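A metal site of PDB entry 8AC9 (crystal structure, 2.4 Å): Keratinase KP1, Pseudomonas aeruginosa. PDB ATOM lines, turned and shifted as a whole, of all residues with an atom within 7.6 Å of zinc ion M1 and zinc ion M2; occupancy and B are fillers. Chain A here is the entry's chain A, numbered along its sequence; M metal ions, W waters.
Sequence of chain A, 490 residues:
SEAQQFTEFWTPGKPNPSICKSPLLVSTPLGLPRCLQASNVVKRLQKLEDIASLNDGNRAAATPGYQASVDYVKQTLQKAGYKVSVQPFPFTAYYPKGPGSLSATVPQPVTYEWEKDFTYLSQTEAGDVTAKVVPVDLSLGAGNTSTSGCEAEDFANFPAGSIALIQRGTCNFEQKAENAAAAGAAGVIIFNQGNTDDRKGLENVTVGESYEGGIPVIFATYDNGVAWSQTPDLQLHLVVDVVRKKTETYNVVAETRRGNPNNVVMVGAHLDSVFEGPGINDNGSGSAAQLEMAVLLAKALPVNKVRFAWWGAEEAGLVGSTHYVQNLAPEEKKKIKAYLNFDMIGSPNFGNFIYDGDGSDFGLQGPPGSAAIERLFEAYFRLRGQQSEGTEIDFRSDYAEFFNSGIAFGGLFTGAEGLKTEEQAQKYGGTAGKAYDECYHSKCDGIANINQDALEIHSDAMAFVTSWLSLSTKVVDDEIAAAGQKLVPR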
ATOM      1  N   HIS A 270       4.660  -8.081  10.852  1.00  0.00           N
ATOM      2  CA  HIS A 270       4.610  -9.136  11.865  1.00  0.00           C
ATOM      3  C   HIS A 270       3.235  -9.174  12.530  1.00  0.00           C
ATOM      4  O   HIS A 270       2.590  -8.142  12.760  1.00  0.00           O
ATOM      5  CB  HIS A 270       5.745  -8.987  12.898  1.00  0.00           C
ATOM      6  CG  HIS A 270       5.576  -7.888  13.903  1.00  0.00           C
ATOM      7  ND1 HIS A 270       4.914  -8.057  15.100  1.00  0.00           N
ATOM      8  CD2 HIS A 270       6.083  -6.630  13.938  1.00  0.00           C
ATOM      9  CE1 HIS A 270       4.971  -6.936  15.798  1.00  0.00           C
ATOM     10  NE2 HIS A 270       5.678  -6.056  15.121  1.00  0.00           N
ATOM     11  N   ASP A 272       2.494 -11.175  15.378  1.00  0.00           N
ATOM     12  CA  ASP A 272       2.514 -11.445  16.818  1.00  0.00           C
ATOM     13  C   ASP A 272       2.529 -10.144  17.616  1.00  0.00           C
ATOM     14  O   ASP A 272       2.972  -9.092  17.130  1.00  0.00           O
ATOM     15  CB  ASP A 272       3.717 -12.293  17.228  1.00  0.00           C
ATOM     16  CG  ASP A 272       5.062 -11.619  16.939  1.00  0.00           C
ATOM     17  OD1 ASP A 272       5.223 -11.063  15.824  1.00  0.00           O
ATOM     18  OD2 ASP A 272       5.974 -11.668  17.799  1.00  0.00           O
ATOM     19  N   SER A 273       1.999 -10.236  18.818  1.00  0.00           N
ATOM     20  CA  SER A 273       2.076  -9.195  19.820  1.00  0.00           C
ATOM     21  C   SER A 273       3.077  -9.630  20.888  1.00  0.00           C
ATOM     22  O   SER A 273       3.472 -10.788  20.930  1.00  0.00           O
ATOM     23  CB  SER A 273       0.707  -8.969  20.464  1.00  0.00           C
ATOM     24  OG  SER A 273       0.334 -10.173  21.125  1.00  0.00           O
ATOM     25  N   VAL A 274       3.436  -8.707  21.783  1.00  0.00           N
ATOM     26  CA  VAL A 274       4.151  -9.088  23.007  1.00  0.00           C
ATOM     27  C   VAL A 274       3.179  -9.860  23.893  1.00  0.00           C
ATOM     28  O   VAL A 274       1.966  -9.899  23.630  1.00  0.00           O
ATOM     29  CB  VAL A 274       4.722  -7.886  23.776  1.00  0.00           C
ATOM     30  CG1 VAL A 274       5.886  -7.235  23.015  1.00  0.00           C
ATOM     31  CG2 VAL A 274       3.628  -6.895  24.064  1.00  0.00           C
ATOM     32  N   ASN A 281      -1.915  -1.708  17.780  1.00  0.00           N
ATOM     33  CA  ASN A 281      -1.014  -0.874  16.974  1.00  0.00           C
ATOM     34  C   ASN A 281       0.234  -1.657  16.584  1.00  0.00           C
ATOM     35  O   ASN A 281       0.668  -1.606  15.429  1.00  0.00           O
ATOM     36  CB  ASN A 281      -0.588   0.435  17.664  1.00  0.00           C
ATOM     37  CG  ASN A 281       0.173   1.370  16.679  1.00  0.00           C
ATOM     38  OD1 ASN A 281      -0.195   1.450  15.501  1.00  0.00           O
ATOM     39  ND2 ASN A 281       1.264   2.014  17.147  1.00  0.00           N
ATOM     40  N   ASP A 282       0.817  -2.359  17.553  1.00  0.00           N
ATOM     41  CA  ASP A 282       2.041  -3.137  17.349  1.00  0.00           C
ATOM     42  C   ASP A 282       1.750  -4.642  17.474  1.00  0.00           C
ATOM     43  O   ASP A 282       1.811  -5.195  18.570  1.00  0.00           O
ATOM     44  CB  ASP A 282       3.103  -2.685  18.349  1.00  0.00           C
ATOM     45  CG  ASP A 282       4.410  -3.366  18.128  1.00  0.00           C
ATOM     46  OD1 ASP A 282       4.633  -3.866  17.019  1.00  0.00           O
ATOM     47  OD2 ASP A 282       5.214  -3.430  19.076  1.00  0.00           O
ATOM     48  N   ASN A 283       1.491  -5.310  16.344  1.00  0.00           N
ATOM     49  CA  ASN A 283       1.467  -4.696  15.017  1.00  0.00           C
ATOM     50  C   ASN A 283       0.232  -5.149  14.256  1.00  0.00           C
ATOM     51  O   ASN A 283       0.316  -5.526  13.072  1.00  0.00           O
ATOM     52  CB  ASN A 283       2.740  -5.023  14.211  1.00  0.00           C
ATOM     53  CG  ASN A 283       2.751  -4.355  12.818  1.00  0.00           C
ATOM     54  OD1 ASN A 283       2.330  -3.202  12.668  1.00  0.00           O
ATOM     55  ND2 ASN A 283       3.207  -5.093  11.807  1.00  0.00           N
ATOM     56  N   GLY A 284      -0.902  -5.125  14.914  1.00  0.00           N
ATOM     57  CA  GLY A 284      -2.148  -5.301  14.187  1.00  0.00           C
ATOM     58  C   GLY A 284      -2.285  -4.317  13.048  1.00  0.00           C
ATOM     59  O   GLY A 284      -2.819  -4.644  11.987  1.00  0.00           O
ATOM     60  N   GLU A 314       8.176 -11.944  15.949  1.00  0.00           N
ATOM     61  CA  GLU A 314       9.030 -10.782  15.784  1.00  0.00           C
ATOM     62  C   GLU A 314       9.431 -10.206  17.134  1.00  0.00           C
ATOM     63  O   GLU A 314      10.538  -9.691  17.288  1.00  0.00           O
ATOM     64  CB  GLU A 314       8.320  -9.711  14.965  1.00  0.00           C
ATOM     65  CG  GLU A 314       9.175  -8.478  14.710  1.00  0.00           C
ATOM     66  CD  GLU A 314       8.962  -7.393  15.716  1.00  0.00           C
ATOM     67  OE1 GLU A 314       8.066  -7.562  16.588  1.00  0.00           O
ATOM     68  OE2 GLU A 314       9.692  -6.376  15.640  1.00  0.00           O
ATOM     69  N   GLU A 315       8.521 -10.234  18.086  1.00  0.00           N
ATOM     70  CA  GLU A 315       8.772  -9.672  19.402  1.00  0.00           C
ATOM     71  C   GLU A 315       9.772 -10.516  20.202  1.00  0.00           C
ATOM     72  O   GLU A 315      10.276 -10.036  21.211  1.00  0.00           O
ATOM     73  CB  GLU A 315       7.458  -9.544  20.169  1.00  0.00           C
ATOM     74  CG  GLU A 315       6.382  -8.739  19.441  1.00  0.00           C
ATOM     75  CD  GLU A 315       6.663  -7.235  19.452  1.00  0.00           C
ATOM     76  OE1 GLU A 315       7.814  -6.848  19.691  1.00  0.00           O
ATOM     77  OE2 GLU A 315       5.734  -6.447  19.234  1.00  0.00           O
ATOM     78  N   ASN A 341       8.264  -3.055   4.553  1.00  0.00           N
ATOM     79  CA  ASN A 341       7.935  -3.454   5.919  1.00  0.00           C
ATOM     80  C   ASN A 341       6.944  -2.482   6.530  1.00  0.00           C
ATOM     81  O   ASN A 341       7.122  -1.258   6.421  1.00  0.00           O
ATOM     82  CB  ASN A 341       9.202  -3.538   6.774  1.00  0.00           C
ATOM     83  CG  ASN A 341       8.951  -4.227   8.066  1.00  0.00           C
ATOM     84  OD1 ASN A 341       8.577  -5.393   8.100  1.00  0.00           O
ATOM     85  ND2 ASN A 341       9.142  -3.504   9.159  1.00  0.00           N
ATOM     86  N   PHE A 342       5.909  -3.001   7.172  1.00  0.00           N
ATOM     87  CA  PHE A 342       4.902  -2.153   7.807  1.00  0.00           C
ATOM     88  C   PHE A 342       4.701  -2.604   9.247  1.00  0.00           C
ATOM     89  O   PHE A 342       3.981  -3.575   9.519  1.00  0.00           O
ATOM     90  CB  PHE A 342       3.616  -2.171   6.999  1.00  0.00           C
ATOM     91  CG  PHE A 342       3.823  -1.768   5.583  1.00  0.00           C
ATOM     92  CD1 PHE A 342       4.017  -0.429   5.269  1.00  0.00           C
ATOM     93  CD2 PHE A 342       3.953  -2.723   4.592  1.00  0.00           C
ATOM     94  CE1 PHE A 342       4.281  -0.046   3.972  1.00  0.00           C
ATOM     95  CE2 PHE A 342       4.213  -2.354   3.308  1.00  0.00           C
ATOM     96  CZ  PHE A 342       4.376  -1.013   2.987  1.00  0.00           C
ATOM     97  N   ASP A 343       5.323  -1.879  10.170  1.00  0.00           N
ATOM     98  CA  ASP A 343       5.344  -2.235  11.589  1.00  0.00           C
ATOM     99  C   ASP A 343       5.031  -0.987  12.408  1.00  0.00           C
ATOM    100  O   ASP A 343       5.890  -0.121  12.573  1.00  0.00           O
ATOM    101  CB  ASP A 343       6.704  -2.839  11.971  1.00  0.00           C
ATOM    102  CG  ASP A 343       6.729  -3.394  13.395  1.00  0.00           C
ATOM    103  OD1 ASP A 343       5.752  -3.176  14.157  1.00  0.00           O
ATOM    104  OD2 ASP A 343       7.732  -4.070  13.751  1.00  0.00           O
ATOM    105  N   MET A 344       3.812  -0.912  12.926  1.00  0.00           N
ATOM    106  CA  MET A 344       3.332   0.227  13.706  1.00  0.00           C
ATOM    107  C   MET A 344       3.066   1.417  12.792  1.00  0.00           C
ATOM    108  O   MET A 344       3.984   2.201  12.494  1.00  0.00           O
ATOM    109  CB  MET A 344       4.307   0.589  14.840  1.00  0.00           C
ATOM    110  CG  MET A 344       4.623  -0.550  15.843  1.00  0.00           C
ATOM    111  SD  MET A 344       5.565   0.025  17.304  1.00  0.00           S
ATOM    112  CE  MET A 344       4.406   1.210  18.012  1.00  0.00           C
ATOM    113  N   ARG A 396      15.127  -2.976  14.257  1.00  0.00           N
ATOM    114  CA  ARG A 396      14.171  -3.417  15.265  1.00  0.00           C
ATOM    115  C   ARG A 396      12.905  -4.001  14.653  1.00  0.00           C
ATOM    116  O   ARG A 396      11.895  -4.124  15.355  1.00  0.00           O
ATOM    117  CB  ARG A 396      13.813  -2.273  16.229  1.00  0.00           C
ATOM    118  CG  ARG A 396      14.703  -2.215  17.469  1.00  0.00           C
ATOM    119  CD  ARG A 396      14.600  -0.873  18.198  1.00  0.00           C
ATOM    120  NE  ARG A 396      13.355  -0.764  18.965  1.00  0.00           N
ATOM    121  CZ  ARG A 396      12.954   0.349  19.569  1.00  0.00           C
ATOM    122  NH1 ARG A 396      13.697   1.446  19.512  1.00  0.00           N
ATOM    123  NH2 ARG A 396      11.812   0.364  20.247  1.00  0.00           N
ATOM    124  N   SER A 397      12.955  -4.391  13.382  1.00  0.00           N
ATOM    125  CA  SER A 397      11.816  -5.058  12.764  1.00  0.00           C
ATOM    126  C   SER A 397      12.319  -5.989  11.670  1.00  0.00           C
ATOM    127  O   SER A 397      13.526  -6.177  11.484  1.00  0.00           O
ATOM    128  CB  SER A 397      10.818  -4.033  12.203  1.00  0.00           C
ATOM    129  OG  SER A 397       9.513  -4.597  12.101  1.00  0.00           O
ATOM    130  N   ASP A 398      11.379  -6.522  10.880  1.00  0.00           N
ATOM    131  CA  ASP A 398      11.583  -7.707  10.083  1.00  0.00           C
ATOM    132  C   ASP A 398      12.322  -7.457   8.772  1.00  0.00           C
ATOM    133  O   ASP A 398      12.641  -8.411   8.060  1.00  0.00           O
ATOM    134  CB  ASP A 398      10.234  -8.357   9.821  1.00  0.00           C
ATOM    135  CG  ASP A 398       9.630  -8.939  11.091  1.00  0.00           C
ATOM    136  OD1 ASP A 398      10.208  -9.895  11.642  1.00  0.00           O
ATOM    137  OD2 ASP A 398       8.602  -8.416  11.547  1.00  0.00           O
ATOM    138  N   PHE A 413       6.504   3.895   9.476  1.00  0.00           N
ATOM    139  CA  PHE A 413       6.553   3.787  10.923  1.00  0.00           C
ATOM    140  C   PHE A 413       5.916   5.058  11.478  1.00  0.00           C
ATOM    141  O   PHE A 413       6.183   6.141  10.955  1.00  0.00           O
ATOM    142  CB  PHE A 413       8.010   3.618  11.370  1.00  0.00           C
ATOM    143  CG  PHE A 413       8.225   3.519  12.865  1.00  0.00           C
ATOM    144  CD1 PHE A 413       7.419   2.719  13.649  1.00  0.00           C
ATOM    145  CD2 PHE A 413       9.274   4.216  13.474  1.00  0.00           C
ATOM    146  CE1 PHE A 413       7.645   2.614  15.032  1.00  0.00           C
ATOM    147  CE2 PHE A 413       9.517   4.120  14.842  1.00  0.00           C
ATOM    148  CZ  PHE A 413       8.716   3.313  15.619  1.00  0.00           C
ATOM    149  N   ALA A 416       7.246   4.749  18.242  1.00  0.00           N
ATOM    150  CA  ALA A 416       6.985   3.887  19.378  1.00  0.00           C
ATOM    151  C   ALA A 416       7.225   4.632  20.684  1.00  0.00           C
ATOM    152  O   ALA A 416       6.466   5.556  21.018  1.00  0.00           O
ATOM    153  CB  ALA A 416       7.828   2.627  19.292  1.00  0.00           C
ATOM    154  N   TYR A 440       2.894   1.520  23.950  1.00  0.00           N
ATOM    155  CA  TYR A 440       3.838   0.591  23.374  1.00  0.00           C
ATOM    156  C   TYR A 440       4.035  -0.644  24.260  1.00  0.00           C
ATOM    157  O   TYR A 440       4.377  -0.542  25.436  1.00  0.00           O
ATOM    158  CB  TYR A 440       5.156   1.340  23.164  1.00  0.00           C
ATOM    159  CG  TYR A 440       6.223   0.522  22.536  1.00  0.00           C
ATOM    160  CD1 TYR A 440       6.022  -0.096  21.295  1.00  0.00           C
ATOM    161  CD2 TYR A 440       7.442   0.343  23.174  1.00  0.00           C
ATOM    162  CE1 TYR A 440       7.020  -0.867  20.700  1.00  0.00           C
ATOM    163  CE2 TYR A 440       8.456  -0.433  22.594  1.00  0.00           C
ATOM    164  CZ  TYR A 440       8.236  -1.025  21.361  1.00  0.00           C
ATOM    165  OH  TYR A 440       9.215  -1.791  20.781  1.00  0.00           O
ATOM    166  N   HIS A 441       3.803  -1.825  23.686  1.00  0.00           N
ATOM    167  CA  HIS A 441       4.085  -3.093  24.359  1.00  0.00           C
ATOM    168  C   HIS A 441       3.310  -3.220  25.660  1.00  0.00           C
ATOM    169  O   HIS A 441       3.775  -3.860  26.600  1.00  0.00           O
ATOM    170  CB  HIS A 441       5.587  -3.264  24.599  1.00  0.00           C
ATOM    171  CG  HIS A 441       6.348  -3.688  23.376  1.00  0.00           C
ATOM    172  ND1 HIS A 441       7.653  -4.132  23.411  1.00  0.00           N
ATOM    173  CD2 HIS A 441       5.974  -3.746  22.070  1.00  0.00           C
ATOM    174  CE1 HIS A 441       8.051  -4.443  22.186  1.00  0.00           C
ATOM    175  NE2 HIS A 441       7.044  -4.222  21.354  1.00  0.00           N
ATOM    176  N   ASP A 445      -2.511  -1.383  24.481  1.00  0.00           N
ATOM    177  CA  ASP A 445      -2.329  -1.271  23.019  1.00  0.00           C
ATOM    178  C   ASP A 445      -3.480  -1.997  22.329  1.00  0.00           C
ATOM    179  O   ASP A 445      -3.324  -3.030  21.676  1.00  0.00           O
ATOM    180  CB  ASP A 445      -0.973  -1.825  22.570  1.00  0.00           C
ATOM    181  CG  ASP A 445      -0.759  -1.723  21.045  1.00  0.00           C
ATOM    182  OD1 ASP A 445      -1.551  -1.005  20.385  1.00  0.00           O
ATOM    183  OD2 ASP A 445       0.183  -2.373  20.508  1.00  0.00           O
HETATM  184 ZN    ZN M   1       6.290  -4.305  15.896  1.00  0.00          ZN
HETATM  185 ZN    ZN M   2       6.984  -4.628  19.188  1.00  0.00          ZN
HETATM  186  O   HOH W   1       7.814  -5.191  17.314  1.00  0.00           O
HETATM  187  O   HOH W   2       8.899  -3.376  18.642  1.00  0.00           O
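The side-chain carboxylate (OD2) of Asp 272 sits at hydrogen-bond distance from the backbone NH (N) of Glu 315 (2.9 Å). The side-chain carboxylate (OD2) of Asp 445 sits at hydrogen-bond distance from the backbone NH (N) of Asp 282. The backbone carbonyl oxygen (O) of Phe 342 lies within hydrogen-bond range of the side-chain amide nitrogen (ND2) of Asn 283 (2.9 Å). A ring nitrogen (NE2) of His 441 lies close to the side-chain hydroxyl (OH) of Tyr 440 (3.3 Å). ND2 of Asn 283 lies within hydrogen-bond range of O of His 270 (3.3 Å). NH2 of Arg 396 sits at hydrogen-bond distance from OH of Tyr 440 (3.4 Å). The backbone carbonyl oxygen of Asp 272 lies within hydrogen-bond range of a ring nitrogen (ND1) of His 270 (3.0 Å). NE2 of His 270 sits close to OE1 of Glu 314 (3.2 Å).
CB of Asn 283 touches zinc ion M1 (3.99 Å). Glu 314 touches zinc ion M1 (OE1 to ZN, 3.8 Å). Of the 22 residues printed, 5 come within 4 Å of zinc ion M1. The nearest printed residue that does not touch zinc ion M1 is Glu 315 (4.005 Å).
Tyr 440 touches zinc ion M2 (OH to ZN, 3.9 Å). Along chain A the residues within 4 Å of zinc ion M2 span positions 282 to 441.
Zinc ion M2 is bound by water W1 (2.1 Å), the side-chain carboxylate (OD2) of Asp 282 (2.1 Å), a ring nitrogen (NE2) of His 441 (2.2 Å), the side-chain carboxylate (OE2) of Glu 315 (2.2 Å), water W2 (2.4 Å) and the side-chain carboxylate (OE1) of Glu 315 (2.4 Å). Zinc ion M2 has six donor atoms within binding distance.
Zinc ion M1 is bound by a ring nitrogen (NE2) of His 270 (2.0 Å). OD1 of Asp 282 binds zinc ion M1 (2.0 Å). Zinc ion M1 is bound by the side-chain carboxylate (OD1) of Asp 343 (2.1 Å). Zinc ion M1 is bound by water W1 (2.3 Å). OD2 of Asp 343 is bound to zinc ion M1 (2.6 Å).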
